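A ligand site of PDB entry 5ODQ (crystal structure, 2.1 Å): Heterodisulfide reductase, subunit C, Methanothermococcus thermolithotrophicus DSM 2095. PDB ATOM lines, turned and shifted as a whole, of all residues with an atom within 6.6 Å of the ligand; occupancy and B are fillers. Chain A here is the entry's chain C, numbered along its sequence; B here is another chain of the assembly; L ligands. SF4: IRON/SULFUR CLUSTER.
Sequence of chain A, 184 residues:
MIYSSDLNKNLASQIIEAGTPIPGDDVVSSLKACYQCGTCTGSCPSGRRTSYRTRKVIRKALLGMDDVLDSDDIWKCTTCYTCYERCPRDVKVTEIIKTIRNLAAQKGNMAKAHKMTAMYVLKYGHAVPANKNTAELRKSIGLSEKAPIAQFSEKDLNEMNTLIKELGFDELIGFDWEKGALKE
SG of Cys 37 sits close to OG1 of Thr 39 (3.4 Å).
The backbone NH of Arg 456 of chain B lies within hydrogen-bond range of the backbone carbonyl oxygen of Cys 37 (2.9 Å).
NH2 of Arg 55 lies within hydrogen-bond range of OE1 of Gln 36 (3.0 Å).
The side-chain hydroxyl (OH) of Tyr 35 lies close to the side-chain sulfur (SD) of Met 428 of chain B, at 3.7 Å.
The side-chain sulfur (SG) of Cys 87 sits close to the backbone NH (N) of Asp 90.
The backbone NH (N) of Arg 89 lies close to the side-chain sulfur (SG) of Cys 87, 3.3 Å away.
NH1 of Arg 89 sits at hydrogen-bond distance from O of Ala 33 (2.7 Å).
SG of Cys 87 lies close to N of Val 91 (3.3 Å).
Merely in contact with the ligand: Gln 36 (3.5 Å), Thr 39 (3.8 Å), Arg 55 (3.5 Å), Arg 89 (3.9 Å), Val 91 (3.7 Å) and Val 93 (3.6 Å).
Hydrophobic or aromatic side chains within 4 Å of the ligand: Tyr 35, Val 91 and Val 93.
Of the 25 residues printed, 12 come within 4 Å of the ligand.
The backbone NH (N) of Cys 40 lies close to a sulfur (S3) of the ligand (3.4 Å).
The side-chain sulfur (SG) of Cys 40 binds an iron atom (FE4) of the ligand (2.4 Å).
A sulfur (S4) of the ligand sits close to the backbone NH (N) of Tyr 35.
FE2 of the ligand is bound by SG of Cys 37, at 2.3 Å.
N of Cys 37 lies close to S1 of the ligand (3.2 Å).
An iron atom (FE3) of the ligand is bound by the side-chain sulfur (SG) of Cys 34 (2.3 Å).
FE1 of the ligand is bound by SG of Cys 87 (2.4 Å).
N of Gly 38 lies close to S1 of the ligand, at 3.4 Å.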
ATOM      1  N   LEU A  31      29.344 -17.896  13.233  1.00  0.00           N
ATOM      2  CA  LEU A  31      28.889 -19.036  12.427  1.00  0.00           C
ATOM      3  C   LEU A  31      28.390 -20.166  13.313  1.00  0.00           C
ATOM      4  O   LEU A  31      27.505 -20.926  12.920  1.00  0.00           O
ATOM      5  CB  LEU A  31      29.988 -19.552  11.449  1.00  0.00           C
ATOM      6  CG  LEU A  31      31.273 -20.142  12.055  1.00  0.00           C
ATOM      7  CD1 LEU A  31      31.175 -21.648  12.214  1.00  0.00           C
ATOM      8  CD2 LEU A  31      32.462 -19.882  11.140  1.00  0.00           C
ATOM      9  N   ALA A  33      26.494 -19.878  15.784  1.00  0.00           N
ATOM     10  CA  ALA A  33      25.131 -19.555  16.202  1.00  0.00           C
ATOM     11  C   ALA A  33      24.089 -19.995  15.167  1.00  0.00           C
ATOM     12  O   ALA A  33      22.912 -20.041  15.474  1.00  0.00           O
ATOM     13  CB  ALA A  33      24.989 -18.056  16.429  1.00  0.00           C
ATOM     14  N   CYS A  34      24.527 -20.321  13.946  1.00  0.00           N
ATOM     15  CA  CYS A  34      23.622 -20.723  12.858  1.00  0.00           C
ATOM     16  C   CYS A  34      22.743 -21.912  13.196  1.00  0.00           C
ATOM     17  O   CYS A  34      23.257 -22.936  13.628  1.00  0.00           O
ATOM     18  CB  CYS A  34      24.415 -20.990  11.591  1.00  0.00           C
ATOM     19  SG  CYS A  34      23.421 -21.656  10.225  1.00  0.00           S
ATOM     20  N   TYR A  35      21.428 -21.780  12.978  1.00  0.00           N
ATOM     21  CA  TYR A  35      20.522 -22.901  13.220  1.00  0.00           C
ATOM     22  C   TYR A  35      19.875 -23.388  11.916  1.00  0.00           C
ATOM     23  O   TYR A  35      18.777 -23.945  11.935  1.00  0.00           O
ATOM     24  CB  TYR A  35      19.524 -22.679  14.367  1.00  0.00           C
ATOM     25  CG  TYR A  35      18.633 -21.444  14.340  1.00  0.00           C
ATOM     26  CD1 TYR A  35      18.439 -20.723  13.180  1.00  0.00           C
ATOM     27  CD2 TYR A  35      17.937 -21.049  15.476  1.00  0.00           C
ATOM     28  CE1 TYR A  35      17.619 -19.604  13.144  1.00  0.00           C
ATOM     29  CE2 TYR A  35      17.104 -19.944  15.461  1.00  0.00           C
ATOM     30  CZ  TYR A  35      16.951 -19.219  14.301  1.00  0.00           C
ATOM     31  OH  TYR A  35      16.112 -18.130  14.292  1.00  0.00           O
ATOM     32  N   GLN A  36      20.579 -23.178  10.798  1.00  0.00           N
ATOM     33  CA  GLN A  36      20.160 -23.623   9.471  1.00  0.00           C
ATOM     34  C   GLN A  36      18.706 -23.277   9.112  1.00  0.00           C
ATOM     35  O   GLN A  36      17.993 -24.139   8.610  1.00  0.00           O
ATOM     36  CB  GLN A  36      20.359 -25.141   9.383  1.00  0.00           C
ATOM     37  CG  GLN A  36      21.819 -25.544   9.512  1.00  0.00           C
ATOM     38  CD  GLN A  36      22.551 -25.239   8.246  1.00  0.00           C
ATOM     39  OE1 GLN A  36      22.360 -25.899   7.232  1.00  0.00           O
ATOM     40  NE2 GLN A  36      23.349 -24.175   8.265  1.00  0.00           N
ATOM     41  N   CYS A  37      18.280 -22.042   9.327  1.00  0.00           N
ATOM     42  CA  CYS A  37      16.918 -21.643   9.014  1.00  0.00           C
ATOM     43  C   CYS A  37      16.634 -21.443   7.514  1.00  0.00           C
ATOM     44  O   CYS A  37      15.507 -21.660   7.074  1.00  0.00           O
ATOM     45  CB  CYS A  37      16.524 -20.401   9.815  1.00  0.00           C
ATOM     46  SG  CYS A  37      17.365 -18.884   9.305  1.00  0.00           S
ATOM     47  N   GLY A  38      17.633 -21.021   6.738  1.00  0.00           N
ATOM     48  CA  GLY A  38      17.455 -20.803   5.306  1.00  0.00           C
ATOM     49  C   GLY A  38      17.187 -19.369   4.887  1.00  0.00           C
ATOM     50  O   GLY A  38      17.169 -19.079   3.693  1.00  0.00           O
ATOM     51  N   THR A  39      16.964 -18.454   5.848  1.00  0.00           N
ATOM     52  CA  THR A  39      16.695 -17.040   5.539  1.00  0.00           C
ATOM     53  C   THR A  39      17.792 -16.460   4.625  1.00  0.00           C
ATOM     54  O   THR A  39      17.484 -15.692   3.728  1.00  0.00           O
ATOM     55  CB  THR A  39      16.552 -16.226   6.849  1.00  0.00           C
ATOM     56  OG1 THR A  39      15.435 -16.726   7.574  1.00  0.00           O
ATOM     57  CG2 THR A  39      16.361 -14.736   6.604  1.00  0.00           C
ATOM     58  N   CYS A  40      19.047 -16.843   4.853  1.00  0.00           N
ATOM     59  CA  CYS A  40      20.162 -16.371   4.040  1.00  0.00           C
ATOM     60  C   CYS A  40      20.031 -16.818   2.582  1.00  0.00           C
ATOM     61  O   CYS A  40      20.218 -16.016   1.668  1.00  0.00           O
ATOM     62  CB  CYS A  40      21.500 -16.805   4.633  1.00  0.00           C
ATOM     63  SG  CYS A  40      21.595 -18.577   5.028  1.00  0.00           S
ATOM     64  N   THR A  41      19.699 -18.105   2.361  1.00  0.00           N
ATOM     65  CA  THR A  41      19.553 -18.654   1.007  1.00  0.00           C
ATOM     66  C   THR A  41      18.375 -18.016   0.268  1.00  0.00           C
ATOM     67  O   THR A  41      18.481 -17.708  -0.913  1.00  0.00           O
ATOM     68  CB  THR A  41      19.365 -20.160   1.091  1.00  0.00           C
ATOM     69  OG1 THR A  41      20.333 -20.714   1.979  1.00  0.00           O
ATOM     70  CG2 THR A  41      19.487 -20.821  -0.280  1.00  0.00           C
ATOM     71  N   THR A  54      23.584 -20.378   0.306  1.00  0.00           N
ATOM     72  CA  THR A  54      24.307 -19.775   1.419  1.00  0.00           C
ATOM     73  C   THR A  54      24.300 -20.646   2.687  1.00  0.00           C
ATOM     74  O   THR A  54      25.349 -20.857   3.284  1.00  0.00           O
ATOM     75  CB  THR A  54      23.732 -18.397   1.698  1.00  0.00           C
ATOM     76  OG1 THR A  54      23.579 -17.696   0.463  1.00  0.00           O
ATOM     77  CG2 THR A  54      24.589 -17.594   2.647  1.00  0.00           C
ATOM     78  N   ARG A  55      23.134 -21.152   3.088  1.00  0.00           N
ATOM     79  CA  ARG A  55      23.009 -21.992   4.284  1.00  0.00           C
ATOM     80  C   ARG A  55      23.951 -23.216   4.226  1.00  0.00           C
ATOM     81  O   ARG A  55      24.520 -23.573   5.253  1.00  0.00           O
ATOM     82  CB  ARG A  55      21.552 -22.455   4.465  1.00  0.00           C
ATOM     83  CG  ARG A  55      21.314 -23.292   5.728  1.00  0.00           C
ATOM     84  CD  ARG A  55      20.009 -24.064   5.712  1.00  0.00           C
ATOM     85  NE  ARG A  55      19.716 -24.627   4.391  1.00  0.00           N
ATOM     86  CZ  ARG A  55      20.125 -25.821   3.953  1.00  0.00           C
ATOM     87  NH1 ARG A  55      19.794 -26.229   2.736  1.00  0.00           N
ATOM     88  NH2 ARG A  55      20.852 -26.604   4.725  1.00  0.00           N
ATOM     89  N   ILE A  58      27.657 -22.534   5.324  1.00  0.00           N
ATOM     90  CA  ILE A  58      27.771 -22.515   6.783  1.00  0.00           C
ATOM     91  C   ILE A  58      27.644 -23.940   7.339  1.00  0.00           C
ATOM     92  O   ILE A  58      28.318 -24.262   8.311  1.00  0.00           O
ATOM     93  CB  ILE A  58      26.696 -21.573   7.404  1.00  0.00           C
ATOM     94  CG1 ILE A  58      26.677 -20.175   6.728  1.00  0.00           C
ATOM     95  CG2 ILE A  58      26.908 -21.436   8.920  1.00  0.00           C
ATOM     96  CD1 ILE A  58      27.979 -19.415   6.764  1.00  0.00           C
ATOM     97  N   CYS A  83      21.663 -11.273   3.623  1.00  0.00           N
ATOM     98  CA  CYS A  83      21.647 -12.356   4.603  1.00  0.00           C
ATOM     99  C   CYS A  83      22.139 -11.809   5.950  1.00  0.00           C
ATOM    100  O   CYS A  83      21.534 -12.069   6.978  1.00  0.00           O
ATOM    101  CB  CYS A  83      22.529 -13.508   4.112  1.00  0.00           C
ATOM    102  SG  CYS A  83      24.218 -13.007   3.686  1.00  0.00           S
ATOM    103  N   ARG A  86      19.358  -9.903   7.607  1.00  0.00           N
ATOM    104  CA  ARG A  86      18.157 -10.647   8.004  1.00  0.00           C
ATOM    105  C   ARG A  86      18.349 -11.856   8.920  1.00  0.00           C
ATOM    106  O   ARG A  86      17.366 -12.334   9.463  1.00  0.00           O
ATOM    107  CB  ARG A  86      17.428 -11.114   6.729  1.00  0.00           C
ATOM    108  CG  ARG A  86      16.813  -9.962   5.936  1.00  0.00           C
ATOM    109  CD  ARG A  86      16.191 -10.444   4.650  1.00  0.00           C
ATOM    110  NE  ARG A  86      15.746  -9.343   3.801  1.00  0.00           N
ATOM    111  CZ  ARG A  86      15.441  -9.457   2.515  1.00  0.00           C
ATOM    112  NH1 ARG A  86      15.531 -10.627   1.903  1.00  0.00           N
ATOM    113  NH2 ARG A  86      15.030  -8.400   1.821  1.00  0.00           N
ATOM    114  N   CYS A  87      19.573 -12.344   9.122  1.00  0.00           N
ATOM    115  CA  CYS A  87      19.772 -13.512   9.974  1.00  0.00           C
ATOM    116  C   CYS A  87      19.219 -13.349  11.397  1.00  0.00           C
ATOM    117  O   CYS A  87      19.695 -12.504  12.147  1.00  0.00           O
ATOM    118  CB  CYS A  87      21.242 -13.921  10.000  1.00  0.00           C
ATOM    119  SG  CYS A  87      21.618 -15.235  11.199  1.00  0.00           S
ATOM    120  N   PRO A  88      18.242 -14.184  11.793  1.00  0.00           N
ATOM    121  CA  PRO A  88      17.710 -14.075  13.153  1.00  0.00           C
ATOM    122  C   PRO A  88      18.671 -14.546  14.250  1.00  0.00           C
ATOM    123  O   PRO A  88      18.390 -14.332  15.433  1.00  0.00           O
ATOM    124  CB  PRO A  88      16.471 -14.970  13.102  1.00  0.00           C
ATOM    125  CG  PRO A  88      16.820 -16.000  12.101  1.00  0.00           C
ATOM    126  CD  PRO A  88      17.558 -15.253  11.039  1.00  0.00           C
ATOM    127  N   ARG A  89      19.799 -15.184  13.893  1.00  0.00           N
ATOM    128  CA  ARG A  89      20.772 -15.669  14.880  1.00  0.00           C
ATOM    129  C   ARG A  89      22.013 -14.774  14.991  1.00  0.00           C
ATOM    130  O   ARG A  89      22.947 -15.138  15.699  1.00  0.00           O
ATOM    131  CB  ARG A  89      21.148 -17.123  14.569  1.00  0.00           C
ATOM    132  CG  ARG A  89      20.280 -18.126  15.313  1.00  0.00           C
ATOM    133  CD  ARG A  89      20.703 -18.201  16.774  1.00  0.00           C
ATOM    134  NE  ARG A  89      19.845 -19.074  17.577  1.00  0.00           N
ATOM    135  CZ  ARG A  89      20.107 -20.341  17.877  1.00  0.00           C
ATOM    136  NH1 ARG A  89      21.203 -20.926  17.429  1.00  0.00           N
ATOM    137  NH2 ARG A  89      19.256 -21.044  18.618  1.00  0.00           N
ATOM    138  N   ASP A  90      22.024 -13.625  14.305  1.00  0.00           N
ATOM    139  CA  ASP A  90      23.146 -12.666  14.328  1.00  0.00           C
ATOM    140  C   ASP A  90      24.400 -13.234  13.711  1.00  0.00           C
ATOM    141  O   ASP A  90      25.508 -12.835  14.081  1.00  0.00           O
ATOM    142  CB  ASP A  90      23.388 -12.110  15.747  1.00  0.00           C
ATOM    143  CG  ASP A  90      22.573 -10.870  16.070  1.00  0.00           C
ATOM    144  OD1 ASP A  90      22.066 -10.226  15.126  1.00  0.00           O
ATOM    145  OD2 ASP A  90      22.462 -10.525  17.267  1.00  0.00           O
ATOM    146  N   VAL A  91      24.260 -14.156  12.769  1.00  0.00           N
ATOM    147  CA  VAL A  91      25.409 -14.721  12.108  1.00  0.00           C
ATOM    148  C   VAL A  91      25.859 -13.602  11.172  1.00  0.00           C
ATOM    149  O   VAL A  91      25.027 -12.925  10.571  1.00  0.00           O
ATOM    150  CB  VAL A  91      25.066 -16.022  11.337  1.00  0.00           C
ATOM    151  CG1 VAL A  91      26.295 -16.560  10.590  1.00  0.00           C
ATOM    152  CG2 VAL A  91      24.511 -17.089  12.281  1.00  0.00           C
ATOM    153  N   LYS A  92      27.159 -13.364  11.076  1.00  0.00           N
ATOM    154  CA  LYS A  92      27.706 -12.309  10.225  1.00  0.00           C
ATOM    155  C   LYS A  92      28.118 -13.049   8.981  1.00  0.00           C
ATOM    156  O   LYS A  92      29.296 -13.152   8.649  1.00  0.00           O
ATOM    157  CB  LYS A  92      28.880 -11.622  10.944  1.00  0.00           C
ATOM    158  CG  LYS A  92      28.547 -11.155  12.377  1.00  0.00           C
ATOM    159  CD  LYS A  92      27.610  -9.936  12.406  1.00  0.00           C
ATOM    160  CE  LYS A  92      27.433  -9.369  13.803  1.00  0.00           C
ATOM    161  NZ  LYS A  92      26.404 -10.114  14.597  1.00  0.00           N
ATOM    162  N   VAL A  93      27.102 -13.584   8.294  1.00  0.00           N
ATOM    163  CA  VAL A  93      27.218 -14.402   7.100  1.00  0.00           C
ATOM    164  C   VAL A  93      28.228 -13.868   6.071  1.00  0.00           C
ATOM    165  O   VAL A  93      29.180 -14.577   5.737  1.00  0.00           O
ATOM    166  CB  VAL A  93      25.833 -14.665   6.438  1.00  0.00           C
ATOM    167  CG1 VAL A  93      25.940 -15.795   5.420  1.00  0.00           C
ATOM    168  CG2 VAL A  93      24.769 -15.016   7.485  1.00  0.00           C
ATOM    169  N   MET B 428      10.944 -23.935  11.294  1.00  0.00           N
ATOM    170  CA  MET B 428      12.349 -24.283  11.572  1.00  0.00           C
ATOM    171  C   MET B 428      12.307 -25.560  12.401  1.00  0.00           C
ATOM    172  O   MET B 428      12.928 -26.552  12.061  1.00  0.00           O
ATOM    173  CB  MET B 428      13.039 -23.166  12.364  1.00  0.00           C
ATOM    174  CG  MET B 428      13.495 -22.024  11.488  1.00  0.00           C
ATOM    175  SD  MET B 428      14.421 -20.794  12.428  1.00  0.00           S
ATOM    176  CE  MET B 428      13.132 -20.035  13.301  1.00  0.00           C
ATOM    177  N   ARG B 456      12.685 -20.840   7.138  1.00  0.00           N
ATOM    178  CA  ARG B 456      12.203 -19.584   7.652  1.00  0.00           C
ATOM    179  C   ARG B 456      12.177 -18.637   6.464  1.00  0.00           C
ATOM    180  O   ARG B 456      13.214 -18.384   5.855  1.00  0.00           O
ATOM    181  CB  ARG B 456      13.117 -19.050   8.740  1.00  0.00           C
ATOM    182  CG  ARG B 456      12.652 -17.748   9.334  1.00  0.00           C
ATOM    183  CD  ARG B 456      13.660 -17.243  10.335  1.00  0.00           C
ATOM    184  NE  ARG B 456      13.217 -16.003  10.958  1.00  0.00           N
ATOM    185  CZ  ARG B 456      13.247 -14.813  10.362  1.00  0.00           C
ATOM    186  NH1 ARG B 456      13.694 -14.696   9.116  1.00  0.00           N
ATOM    187  NH2 ARG B 456      12.819 -13.738  11.006  1.00  0.00           N
ATOM    188  N   GLU B 474      13.557 -20.979   1.410  1.00  0.00           N
ATOM    189  CA  GLU B 474      14.307 -22.127   0.946  1.00  0.00           C
ATOM    190  C   GLU B 474      13.710 -23.366   1.551  1.00  0.00           C
ATOM    191  O   GLU B 474      13.515 -23.422   2.765  1.00  0.00           O
ATOM    192  CB  GLU B 474      15.777 -22.065   1.376  1.00  0.00           C
ATOM    193  CG  GLU B 474      16.554 -23.314   0.964  1.00  0.00           C
ATOM    194  CD  GLU B 474      17.914 -23.487   1.579  1.00  0.00           C
ATOM    195  OE1 GLU B 474      18.747 -24.184   0.956  1.00  0.00           O
ATOM    196  OE2 GLU B 474      18.131 -23.024   2.723  1.00  0.00           O
HETATM  197 FE1  SF4 L   1      21.500 -17.259   9.844  1.00  0.00          FE
HETATM  198 FE2  SF4 L   1      19.697 -19.018   9.149  1.00  0.00          FE
HETATM  199 FE3  SF4 L   1      22.123 -19.876   9.644  1.00  0.00          FE
HETATM  200 FE4  SF4 L   1      21.554 -18.486   7.409  1.00  0.00          FE
HETATM  201  S1  SF4 L   1      20.760 -20.564   7.917  1.00  0.00           S
HETATM  202  S2  SF4 L   1      23.324 -18.075   8.840  1.00  0.00           S
HETATM  203  S3  SF4 L   1      20.036 -16.998   8.132  1.00  0.00           S
HETATM  204  S4  SF4 L   1      20.744 -18.976  11.189  1.00  0.00           S
